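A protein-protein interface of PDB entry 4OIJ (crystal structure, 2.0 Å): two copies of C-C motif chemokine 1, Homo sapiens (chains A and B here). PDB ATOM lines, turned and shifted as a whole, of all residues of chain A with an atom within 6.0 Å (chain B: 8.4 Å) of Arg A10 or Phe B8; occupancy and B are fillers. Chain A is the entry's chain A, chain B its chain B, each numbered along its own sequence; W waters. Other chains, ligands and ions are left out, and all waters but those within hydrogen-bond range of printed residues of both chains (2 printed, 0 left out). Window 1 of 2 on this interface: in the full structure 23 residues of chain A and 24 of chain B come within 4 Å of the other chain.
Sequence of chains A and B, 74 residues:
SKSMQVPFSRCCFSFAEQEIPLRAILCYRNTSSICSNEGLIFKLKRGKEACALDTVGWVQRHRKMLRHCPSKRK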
ATOM      1  N   PHE A   8       3.097 -24.616  14.087  1.00  0.00           N
ATOM      2  CA  PHE A   8       2.892 -23.808  12.907  1.00  0.00           C
ATOM      3  C   PHE A   8       4.212 -23.148  12.609  1.00  0.00           C
ATOM      4  O   PHE A   8       5.093 -23.080  13.480  1.00  0.00           O
ATOM      5  CB  PHE A   8       1.764 -22.789  13.096  1.00  0.00           C
ATOM      6  CG  PHE A   8       1.965 -21.842  14.249  1.00  0.00           C
ATOM      7  CD1 PHE A   8       2.799 -20.737  14.125  1.00  0.00           C
ATOM      8  CD2 PHE A   8       1.360 -22.083  15.480  1.00  0.00           C
ATOM      9  CE1 PHE A   8       3.021 -19.885  15.204  1.00  0.00           C
ATOM     10  CE2 PHE A   8       1.576 -21.220  16.564  1.00  0.00           C
ATOM     11  CZ  PHE A   8       2.410 -20.136  16.421  1.00  0.00           C
ATOM     12  N   SER A   9       4.369 -22.697  11.390  1.00  0.00           N
ATOM     13  CA  SER A   9       5.599 -22.034  10.998  1.00  0.00           C
ATOM     14  C   SER A   9       5.353 -20.534  11.122  1.00  0.00           C
ATOM     15  O   SER A   9       4.238 -20.099  10.852  1.00  0.00           O
ATOM     16  CB  SER A   9       5.943 -22.372   9.538  1.00  0.00           C
ATOM     17  OG  SER A   9       6.039 -23.768   9.316  1.00  0.00           O
ATOM     18  N   ARG A  10       6.390 -19.743  11.420  1.00  0.00           N
ATOM     19  CA  ARG A  10       6.289 -18.273  11.440  1.00  0.00           C
ATOM     20  C   ARG A  10       6.925 -17.750  10.173  1.00  0.00           C
ATOM     21  O   ARG A  10       8.143 -17.905   9.976  1.00  0.00           O
ATOM     22  CB  ARG A  10       6.966 -17.652  12.675  1.00  0.00           C
ATOM     23  CG  ARG A  10       6.133 -17.853  13.929  1.00  0.00           C
ATOM     24  CD  ARG A  10       6.710 -17.096  15.117  1.00  0.00           C
ATOM     25  NE  ARG A  10       6.103 -17.543  16.368  1.00  0.00           N
ATOM     26  CZ  ARG A  10       6.436 -18.656  17.008  1.00  0.00           C
ATOM     27  NH1 ARG A  10       5.821 -18.988  18.131  1.00  0.00           N
ATOM     28  NH2 ARG A  10       7.384 -19.450  16.526  1.00  0.00           N
ATOM     29  N   CYS A  11       6.115 -17.172   9.283  1.00  0.00           N
ATOM     30  CA  CYS A  11       6.642 -16.725   7.998  1.00  0.00           C
ATOM     31  C   CYS A  11       6.426 -15.244   7.776  1.00  0.00           C
ATOM     32  O   CYS A  11       5.443 -14.680   8.265  1.00  0.00           O
ATOM     33  CB  CYS A  11       6.048 -17.537   6.859  1.00  0.00           C
ATOM     34  SG  CYS A  11       6.157 -19.327   7.099  1.00  0.00           S
ATOM     35  N   CYS A  12       7.345 -14.633   7.047  1.00  0.00           N
ATOM     36  CA  CYS A  12       7.285 -13.208   6.739  1.00  0.00           C
ATOM     37  C   CYS A  12       7.168 -13.094   5.270  1.00  0.00           C
ATOM     38  O   CYS A  12       8.166 -13.323   4.577  1.00  0.00           O
ATOM     39  CB  CYS A  12       8.545 -12.508   7.234  1.00  0.00           C
ATOM     40  SG  CYS A  12       8.539 -12.177   8.999  1.00  0.00           S
ATOM     41  N   ARG A  29      13.079 -12.816  16.534  1.00  0.00           N
ATOM     42  CA  ARG A  29      12.878 -14.246  16.272  1.00  0.00           C
ATOM     43  C   ARG A  29      13.253 -14.487  14.815  1.00  0.00           C
ATOM     44  O   ARG A  29      13.045 -13.595  13.975  1.00  0.00           O
ATOM     45  CB  ARG A  29      11.396 -14.646  16.440  1.00  0.00           C
ATOM     46  CG  ARG A  29      10.891 -14.767  17.874  1.00  0.00           C
ATOM     47  CD  ARG A  29       9.563 -15.518  17.934  1.00  0.00           C
ATOM     48  NE  ARG A  29       8.837 -15.271  19.184  1.00  0.00           N
ATOM     49  CZ  ARG A  29       8.976 -15.983  20.300  1.00  0.00           C
ATOM     50  NH1 ARG A  29       9.829 -17.000  20.346  1.00  0.00           N
ATOM     51  NH2 ARG A  29       8.273 -15.677  21.379  1.00  0.00           N
ATOM     52  N   ASN A  30      13.769 -15.666  14.500  1.00  0.00           N
ATOM     53  CA  ASN A  30      14.041 -15.996  13.113  1.00  0.00           C
ATOM     54  C   ASN A  30      12.733 -16.556  12.553  1.00  0.00           C
ATOM     55  O   ASN A  30      11.905 -17.064  13.321  1.00  0.00           O
ATOM     56  CB  ASN A  30      15.121 -17.051  13.022  1.00  0.00           C
ATOM     57  CG  ASN A  30      16.480 -16.480  13.250  1.00  0.00           C
ATOM     58  OD1 ASN A  30      17.000 -15.685  12.461  1.00  0.00           O
ATOM     59  ND2 ASN A  30      17.075 -16.862  14.347  1.00  0.00           N
ATOM     60  N   THR A  31      12.529 -16.440  11.239  1.00  0.00           N
ATOM     61  CA  THR A  31      11.361 -17.053  10.593  1.00  0.00           C
ATOM     62  C   THR A  31      11.655 -18.576  10.565  1.00  0.00           C
ATOM     63  O   THR A  31      12.824 -18.969  10.573  1.00  0.00           O
ATOM     64  CB  THR A  31      11.238 -16.574   9.141  1.00  0.00           C
ATOM     65  OG1 THR A  31      12.476 -16.827   8.510  1.00  0.00           O
ATOM     66  CG2 THR A  31      10.914 -15.101   9.019  1.00  0.00           C
ATOM     67  N   SER A  32      10.635 -19.413  10.473  1.00  0.00           N
ATOM     68  CA  SER A  32      10.841 -20.876  10.398  1.00  0.00           C
ATOM     69  C   SER A  32      11.597 -21.210   9.101  1.00  0.00           C
ATOM     70  O   SER A  32      11.340 -20.587   8.059  1.00  0.00           O
ATOM     71  CB  SER A  32       9.506 -21.601  10.440  1.00  0.00           C
ATOM     72  OG  SER A  32       8.767 -21.173  11.567  1.00  0.00           O
ATOM     73  N   CYS A  35      10.166 -21.687   5.387  1.00  0.00           N
ATOM     74  CA  CYS A  35       9.722 -20.471   4.694  1.00  0.00           C
ATOM     75  C   CYS A  35      10.690 -19.307   4.980  1.00  0.00           C
ATOM     76  O   CYS A  35      10.245 -18.154   5.014  1.00  0.00           O
ATOM     77  CB  CYS A  35       8.300 -20.126   5.144  1.00  0.00           C
ATOM     78  SG  CYS A  35       8.153 -19.735   6.915  1.00  0.00           S
ATOM     79  N   ILE A  41      11.937 -11.473  12.411  1.00  0.00           N
ATOM     80  CA  ILE A  41      10.788 -10.898  13.104  1.00  0.00           C
ATOM     81  C   ILE A  41      11.305 -10.065  14.301  1.00  0.00           C
ATOM     82  O   ILE A  41      12.084 -10.572  15.112  1.00  0.00           O
ATOM     83  CB  ILE A  41       9.795 -11.988  13.574  1.00  0.00           C
ATOM     84  CG1 ILE A  41       9.365 -12.905  12.404  1.00  0.00           C
ATOM     85  CG2 ILE A  41       8.581 -11.381  14.325  1.00  0.00           C
ATOM     86  CD1 ILE A  41       8.978 -14.380  12.941  1.00  0.00           C
ATOM     87  N   GLU A  49       4.226  -6.688  16.442  1.00  0.00           N
ATOM     88  CA  GLU A  49       5.300  -7.332  15.659  1.00  0.00           C
ATOM     89  C   GLU A  49       5.623  -6.779  14.269  1.00  0.00           C
ATOM     90  O   GLU A  49       4.803  -6.117  13.615  1.00  0.00           O
ATOM     91  CB  GLU A  49       5.155  -8.849  15.622  1.00  0.00           C
ATOM     92  CG  GLU A  49       6.204  -9.568  16.450  1.00  0.00           C
ATOM     93  CD  GLU A  49       5.702 -10.592  17.444  1.00  0.00           C
ATOM     94  OE1 GLU A  49       4.537 -10.471  17.888  1.00  0.00           O
ATOM     95  OE2 GLU A  49       6.507 -11.464  17.844  1.00  0.00           O
ATOM     96  N   ALA A  50       6.860  -7.019  13.840  1.00  0.00           N
ATOM     97  CA  ALA A  50       7.296  -6.560  12.527  1.00  0.00           C
ATOM     98  C   ALA A  50       8.295  -7.479  11.864  1.00  0.00           C
ATOM     99  O   ALA A  50       9.395  -7.725  12.371  1.00  0.00           O
ATOM    100  CB  ALA A  50       7.837  -5.149  12.594  1.00  0.00           C
ATOM    101  N   CYS A  51       7.899  -7.951  10.688  1.00  0.00           N
ATOM    102  CA  CYS A  51       8.740  -8.687   9.766  1.00  0.00           C
ATOM    103  C   CYS A  51       9.684  -7.687   9.157  1.00  0.00           C
ATOM    104  O   CYS A  51       9.270  -6.587   8.779  1.00  0.00           O
ATOM    105  CB  CYS A  51       7.879  -9.329   8.696  1.00  0.00           C
ATOM    106  SG  CYS A  51       7.061 -10.806   9.269  1.00  0.00           S
ATOM    107  N   GLN B   5       3.529  -1.888  12.525  1.00  0.00           N
ATOM    108  CA  GLN B   5       3.420  -3.358  12.469  1.00  0.00           C
ATOM    109  C   GLN B   5       3.220  -4.002  11.100  1.00  0.00           C
ATOM    110  O   GLN B   5       2.387  -3.558  10.306  1.00  0.00           O
ATOM    111  CB  GLN B   5       2.427  -3.908  13.515  1.00  0.00           C
ATOM    112  CG  GLN B   5       0.975  -3.472  13.339  1.00  0.00           C
ATOM    113  CD  GLN B   5       0.046  -4.335  14.153  1.00  0.00           C
ATOM    114  OE1 GLN B   5      -0.224  -5.495  13.812  1.00  0.00           O
ATOM    115  NE2 GLN B   5      -0.465  -3.787  15.250  1.00  0.00           N
ATOM    116  N   VAL B   6       3.991  -5.087  10.852  1.00  0.00           N
ATOM    117  CA  VAL B   6       4.009  -5.939   9.634  1.00  0.00           C
ATOM    118  C   VAL B   6       4.001  -7.360  10.188  1.00  0.00           C
ATOM    119  O   VAL B   6       5.063  -7.968  10.329  1.00  0.00           O
ATOM    120  CB  VAL B   6       5.245  -5.690   8.721  1.00  0.00           C
ATOM    121  CG1 VAL B   6       4.825  -5.483   7.274  1.00  0.00           C
ATOM    122  CG2 VAL B   6       6.084  -4.526   9.213  1.00  0.00           C
ATOM    123  N   PRO B   7       2.823  -7.856  10.618  1.00  0.00           N
ATOM    124  CA  PRO B   7       2.781  -9.147  11.324  1.00  0.00           C
ATOM    125  C   PRO B   7       3.293 -10.330  10.546  1.00  0.00           C
ATOM    126  O   PRO B   7       3.165 -10.347   9.344  1.00  0.00           O
ATOM    127  CB  PRO B   7       1.294  -9.323  11.667  1.00  0.00           C
ATOM    128  CG  PRO B   7       0.750  -7.946  11.706  1.00  0.00           C
ATOM    129  CD  PRO B   7       1.493  -7.203  10.624  1.00  0.00           C
ATOM    130  N   PHE B   8       3.875 -11.313  11.227  1.00  0.00           N
ATOM    131  CA  PHE B   8       4.313 -12.519  10.575  1.00  0.00           C
ATOM    132  C   PHE B   8       3.058 -13.319  10.287  1.00  0.00           C
ATOM    133  O   PHE B   8       1.990 -13.069  10.871  1.00  0.00           O
ATOM    134  CB  PHE B   8       5.325 -13.307  11.418  1.00  0.00           C
ATOM    135  CG  PHE B   8       4.815 -13.710  12.780  1.00  0.00           C
ATOM    136  CD1 PHE B   8       3.994 -14.820  12.931  1.00  0.00           C
ATOM    137  CD2 PHE B   8       5.115 -12.948  13.905  1.00  0.00           C
ATOM    138  CE1 PHE B   8       3.482 -15.161  14.183  1.00  0.00           C
ATOM    139  CE2 PHE B   8       4.636 -13.313  15.165  1.00  0.00           C
ATOM    140  CZ  PHE B   8       3.815 -14.409  15.293  1.00  0.00           C
ATOM    141  N   SER B   9       3.168 -14.221   9.362  1.00  0.00           N
ATOM    142  CA  SER B   9       2.048 -15.066   8.993  1.00  0.00           C
ATOM    143  C   SER B   9       2.192 -16.371   9.784  1.00  0.00           C
ATOM    144  O   SER B   9       3.320 -16.815   9.988  1.00  0.00           O
ATOM    145  CB  SER B   9       2.095 -15.381   7.493  1.00  0.00           C
ATOM    146  OG  SER B   9       2.156 -14.218   6.692  1.00  0.00           O
ATOM    147  N   ARG B  10       1.078 -17.019  10.131  1.00  0.00           N
ATOM    148  CA  ARG B  10       1.084 -18.335  10.782  1.00  0.00           C
ATOM    149  C   ARG B  10       0.735 -19.368   9.745  1.00  0.00           C
ATOM    150  O   ARG B  10      -0.389 -19.372   9.241  1.00  0.00           O
ATOM    151  CB  ARG B  10       0.101 -18.418  11.972  1.00  0.00           C
ATOM    152  CG  ARG B  10       0.618 -17.651  13.176  1.00  0.00           C
ATOM    153  CD  ARG B  10      -0.206 -17.936  14.428  1.00  0.00           C
ATOM    154  NE  ARG B  10       0.152 -17.017  15.494  1.00  0.00           N
ATOM    155  CZ  ARG B  10      -0.261 -15.760  15.560  1.00  0.00           C
ATOM    156  NH1 ARG B  10      -1.024 -15.253  14.597  1.00  0.00           N
ATOM    157  NH2 ARG B  10       0.117 -14.985  16.563  1.00  0.00           N
ATOM    158  N   CYS B  11       1.704 -20.219   9.385  1.00  0.00           N
ATOM    159  CA  CYS B  11       1.487 -21.198   8.324  1.00  0.00           C
ATOM    160  C   CYS B  11       1.668 -22.611   8.785  1.00  0.00           C
ATOM    161  O   CYS B  11       2.471 -22.869   9.685  1.00  0.00           O
ATOM    162  CB  CYS B  11       2.369 -20.901   7.120  1.00  0.00           C
ATOM    163  SG  CYS B  11       2.305 -19.178   6.567  1.00  0.00           S
ATOM    164  N   CYS B  12       0.908 -23.522   8.178  1.00  0.00           N
ATOM    165  CA  CYS B  12       0.960 -24.941   8.512  1.00  0.00           C
ATOM    166  C   CYS B  12       1.413 -25.645   7.295  1.00  0.00           C
ATOM    167  O   CYS B  12       0.617 -25.778   6.365  1.00  0.00           O
ATOM    168  CB  CYS B  12      -0.418 -25.435   8.933  1.00  0.00           C
ATOM    169  SG  CYS B  12      -0.858 -25.015  10.616  1.00  0.00           S
ATOM    170  N   PHE B  13       2.701 -26.015   7.223  1.00  0.00           N
ATOM    171  CA  PHE B  13       3.197 -26.752   6.052  1.00  0.00           C
ATOM    172  C   PHE B  13       3.312 -28.275   6.362  1.00  0.00           C
ATOM    173  O   PHE B  13       3.571 -29.068   5.459  1.00  0.00           O
ATOM    174  CB  PHE B  13       4.498 -26.160   5.543  1.00  0.00           C
ATOM    175  CG  PHE B  13       4.380 -24.701   5.137  1.00  0.00           C
ATOM    176  CD1 PHE B  13       3.608 -24.326   4.040  1.00  0.00           C
ATOM    177  CD2 PHE B  13       5.095 -23.715   5.809  1.00  0.00           C
ATOM    178  CE1 PHE B  13       3.508 -22.994   3.663  1.00  0.00           C
ATOM    179  CE2 PHE B  13       5.014 -22.392   5.416  1.00  0.00           C
ATOM    180  CZ  PHE B  13       4.227 -22.033   4.342  1.00  0.00           C
ATOM    181  N   SER B  32      -2.829 -17.911   8.410  1.00  0.00           N
ATOM    182  CA  SER B  32      -2.934 -16.627   7.688  1.00  0.00           C
ATOM    183  C   SER B  32      -3.344 -16.902   6.227  1.00  0.00           C
ATOM    184  O   SER B  32      -2.883 -17.892   5.634  1.00  0.00           O
ATOM    185  CB  SER B  32      -1.613 -15.883   7.743  1.00  0.00           C
ATOM    186  OG  SER B  32      -1.188 -15.766   9.093  1.00  0.00           O
ATOM    187  N   ILE B  34      -2.665 -15.681   3.294  1.00  0.00           N
ATOM    188  CA  ILE B  34      -1.624 -15.724   2.244  1.00  0.00           C
ATOM    189  C   ILE B  34      -1.066 -17.141   2.042  1.00  0.00           C
ATOM    190  O   ILE B  34      -0.661 -17.489   0.925  1.00  0.00           O
ATOM    191  CB  ILE B  34      -0.495 -14.680   2.520  1.00  0.00           C
ATOM    192  CG1 ILE B  34       0.457 -14.520   1.305  1.00  0.00           C
ATOM    193  CG2 ILE B  34       0.268 -14.978   3.838  1.00  0.00           C
ATOM    194  CD1 ILE B  34       0.875 -13.118   1.004  1.00  0.00           C
ATOM    195  N   CYS B  35      -1.061 -17.947   3.116  1.00  0.00           N
ATOM    196  CA  CYS B  35      -0.525 -19.315   3.127  1.00  0.00           C
ATOM    197  C   CYS B  35      -1.584 -20.305   3.625  1.00  0.00           C
ATOM    198  O   CYS B  35      -1.214 -21.308   4.245  1.00  0.00           O
ATOM    199  CB  CYS B  35       0.730 -19.370   4.002  1.00  0.00           C
ATOM    200  SG  CYS B  35       0.438 -18.980   5.755  1.00  0.00           S
ATOM    201  N   GLY B  47       1.031 -24.142  26.346  1.00  0.00           N
ATOM    202  CA  GLY B  47       1.459 -23.421  25.151  1.00  0.00           C
ATOM    203  C   GLY B  47       1.856 -24.244  23.941  1.00  0.00           C
ATOM    204  O   GLY B  47       2.431 -23.690  22.997  1.00  0.00           O
ATOM    205  N   GLU B  49       1.314 -26.669  20.430  1.00  0.00           N
ATOM    206  CA  GLU B  49       0.498 -26.446  19.224  1.00  0.00           C
ATOM    207  C   GLU B  49       0.474 -27.540  18.139  1.00  0.00           C
ATOM    208  O   GLU B  49       1.416 -28.339  17.976  1.00  0.00           O
ATOM    209  CB  GLU B  49       0.756 -25.074  18.621  1.00  0.00           C
ATOM    210  CG  GLU B  49      -0.412 -24.114  18.781  1.00  0.00           C
ATOM    211  CD  GLU B  49      -0.119 -22.782  19.435  1.00  0.00           C
ATOM    212  OE1 GLU B  49       0.999 -22.612  19.972  1.00  0.00           O
ATOM    213  OE2 GLU B  49      -1.031 -21.924  19.459  1.00  0.00           O
HETATM  214  O   HOH W   1       4.640 -25.778   9.428  1.00  0.00           O
HETATM  215  O   HOH W   2       4.349  -9.841   7.164  1.00  0.00           O
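Printed residues of chain A that touch a printed residue of chain B: Phe A8, Ser A9, Arg A10, Cys A11, Ile A41, Glu A49, Ala A50 and Cys A51. Hydrophobic or aromatic side chains of chain A within 4 Å of the printed part of chain B: Phe A8, Ile A41 and Ala A50. Among the printed residues, no Asp or Glu carboxylate lies within 4 Å of a Lys or Arg side-chain nitrogen of the other chain.
N of Ser A9 sits at hydrogen-bond distance from O of Cys B11, 2.6 Å away. O of Cys A11 is in hydrogen-bond range of N of Ser B9, at 2.6 Å. The backbone NH (N) of Val B6 lies within hydrogen-bond range of the backbone carbonyl oxygen (O) of Glu A49, 3.1 Å away. The backbone NH (N) of Cys A51 is in hydrogen-bond range of the backbone carbonyl oxygen (O) of Val B6 (2.9 Å). The side-chain sulfur of Cys A51 sits close to the backbone NH of Phe B8, 3.8 Å away.
Arg A10 touches just these residues of chain B: Phe B8 (3.8 Å) and Ser B9 (3.6 Å). Of chain A, only Arg A10 (3.8 Å), Cys A11 (3.4 Å), Ile A41 (3.8 Å), Glu A49 (3.7 Å) and Cys A51 (3.5 Å) come within 4 Å of Phe B8. Of the printed residues of chain A, Cys B11 touches Phe A8 (3.4 Å), Ser A9 (2.6 Å) and Cys A11 (3.9 Å). Of the printed residues of chain A, Phe B13 touches Ser A9 and Cys A11. Ser B32 touches none of the printed residues of chain A. The nearest residue of chain A that does not touch Phe B8 is Cys A12 (4.2 Å).
Water W1 lies within hydrogen-bond range of the side-chain hydroxyl (OG) of Ser A9 (2.5 Å) and the backbone NH (N) of Phe B13 (2.9 Å). Water W2 lies within hydrogen-bond range of O of Pro B7 (2.5 Å) and SG of Cys A51 (3.6 Å).
Among the printed residues, merely in contact across the chains: Phe A8 with Arg B10, Phe A8 with Cys B11, Phe A8 with Glu B49, Ser A9 with Ser B9, Ser A9 with Arg B10, Ser A9 with Phe B13, Arg A10 with Phe B8, Arg A10 with Ser B9, Cys A11 with Phe B8, Cys A11 with Cys B11, Cys A11 with Phe B13, Ile A41 with Phe B8, Glu A49 with Gln B5, Glu A49 with Pro B7, Glu A49 with Phe B8, Ala A50 with Val B6 and Cys A51 with Pro B7.
Phe A8 touches Cys B11, and with the chains exchanged Cys A11 touches Phe B8. Phe A8 touches Glu B49, and with the chains exchanged Glu A49 touches Phe B8. Ser B9 touches its own counterpart, Ser A9. Ser A9 touches Arg B10, and with the chains exchanged Arg A10 touches Ser B9.
OG of Ser A32 sits at hydrogen-bond distance from N of Arg A10, at 2.8 Å. The side-chain sulfur of Cys A11 is disulfide-bonded to the side-chain sulfur of Cys A35, at 2.0 Å. SG of Cys A12 is disulfide-bonded to SG of Cys A51, 2.0 Å away. O of Ile A41 lies within hydrogen-bond range of N of Arg A29, 2.8 Å away. The backbone NH of Arg B10 sits at hydrogen-bond distance from the side-chain hydroxyl of Ser B32 (2.8 Å). SG of Cys B11 is disulfide-bonded to SG of Cys B35 (2.0 Å).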
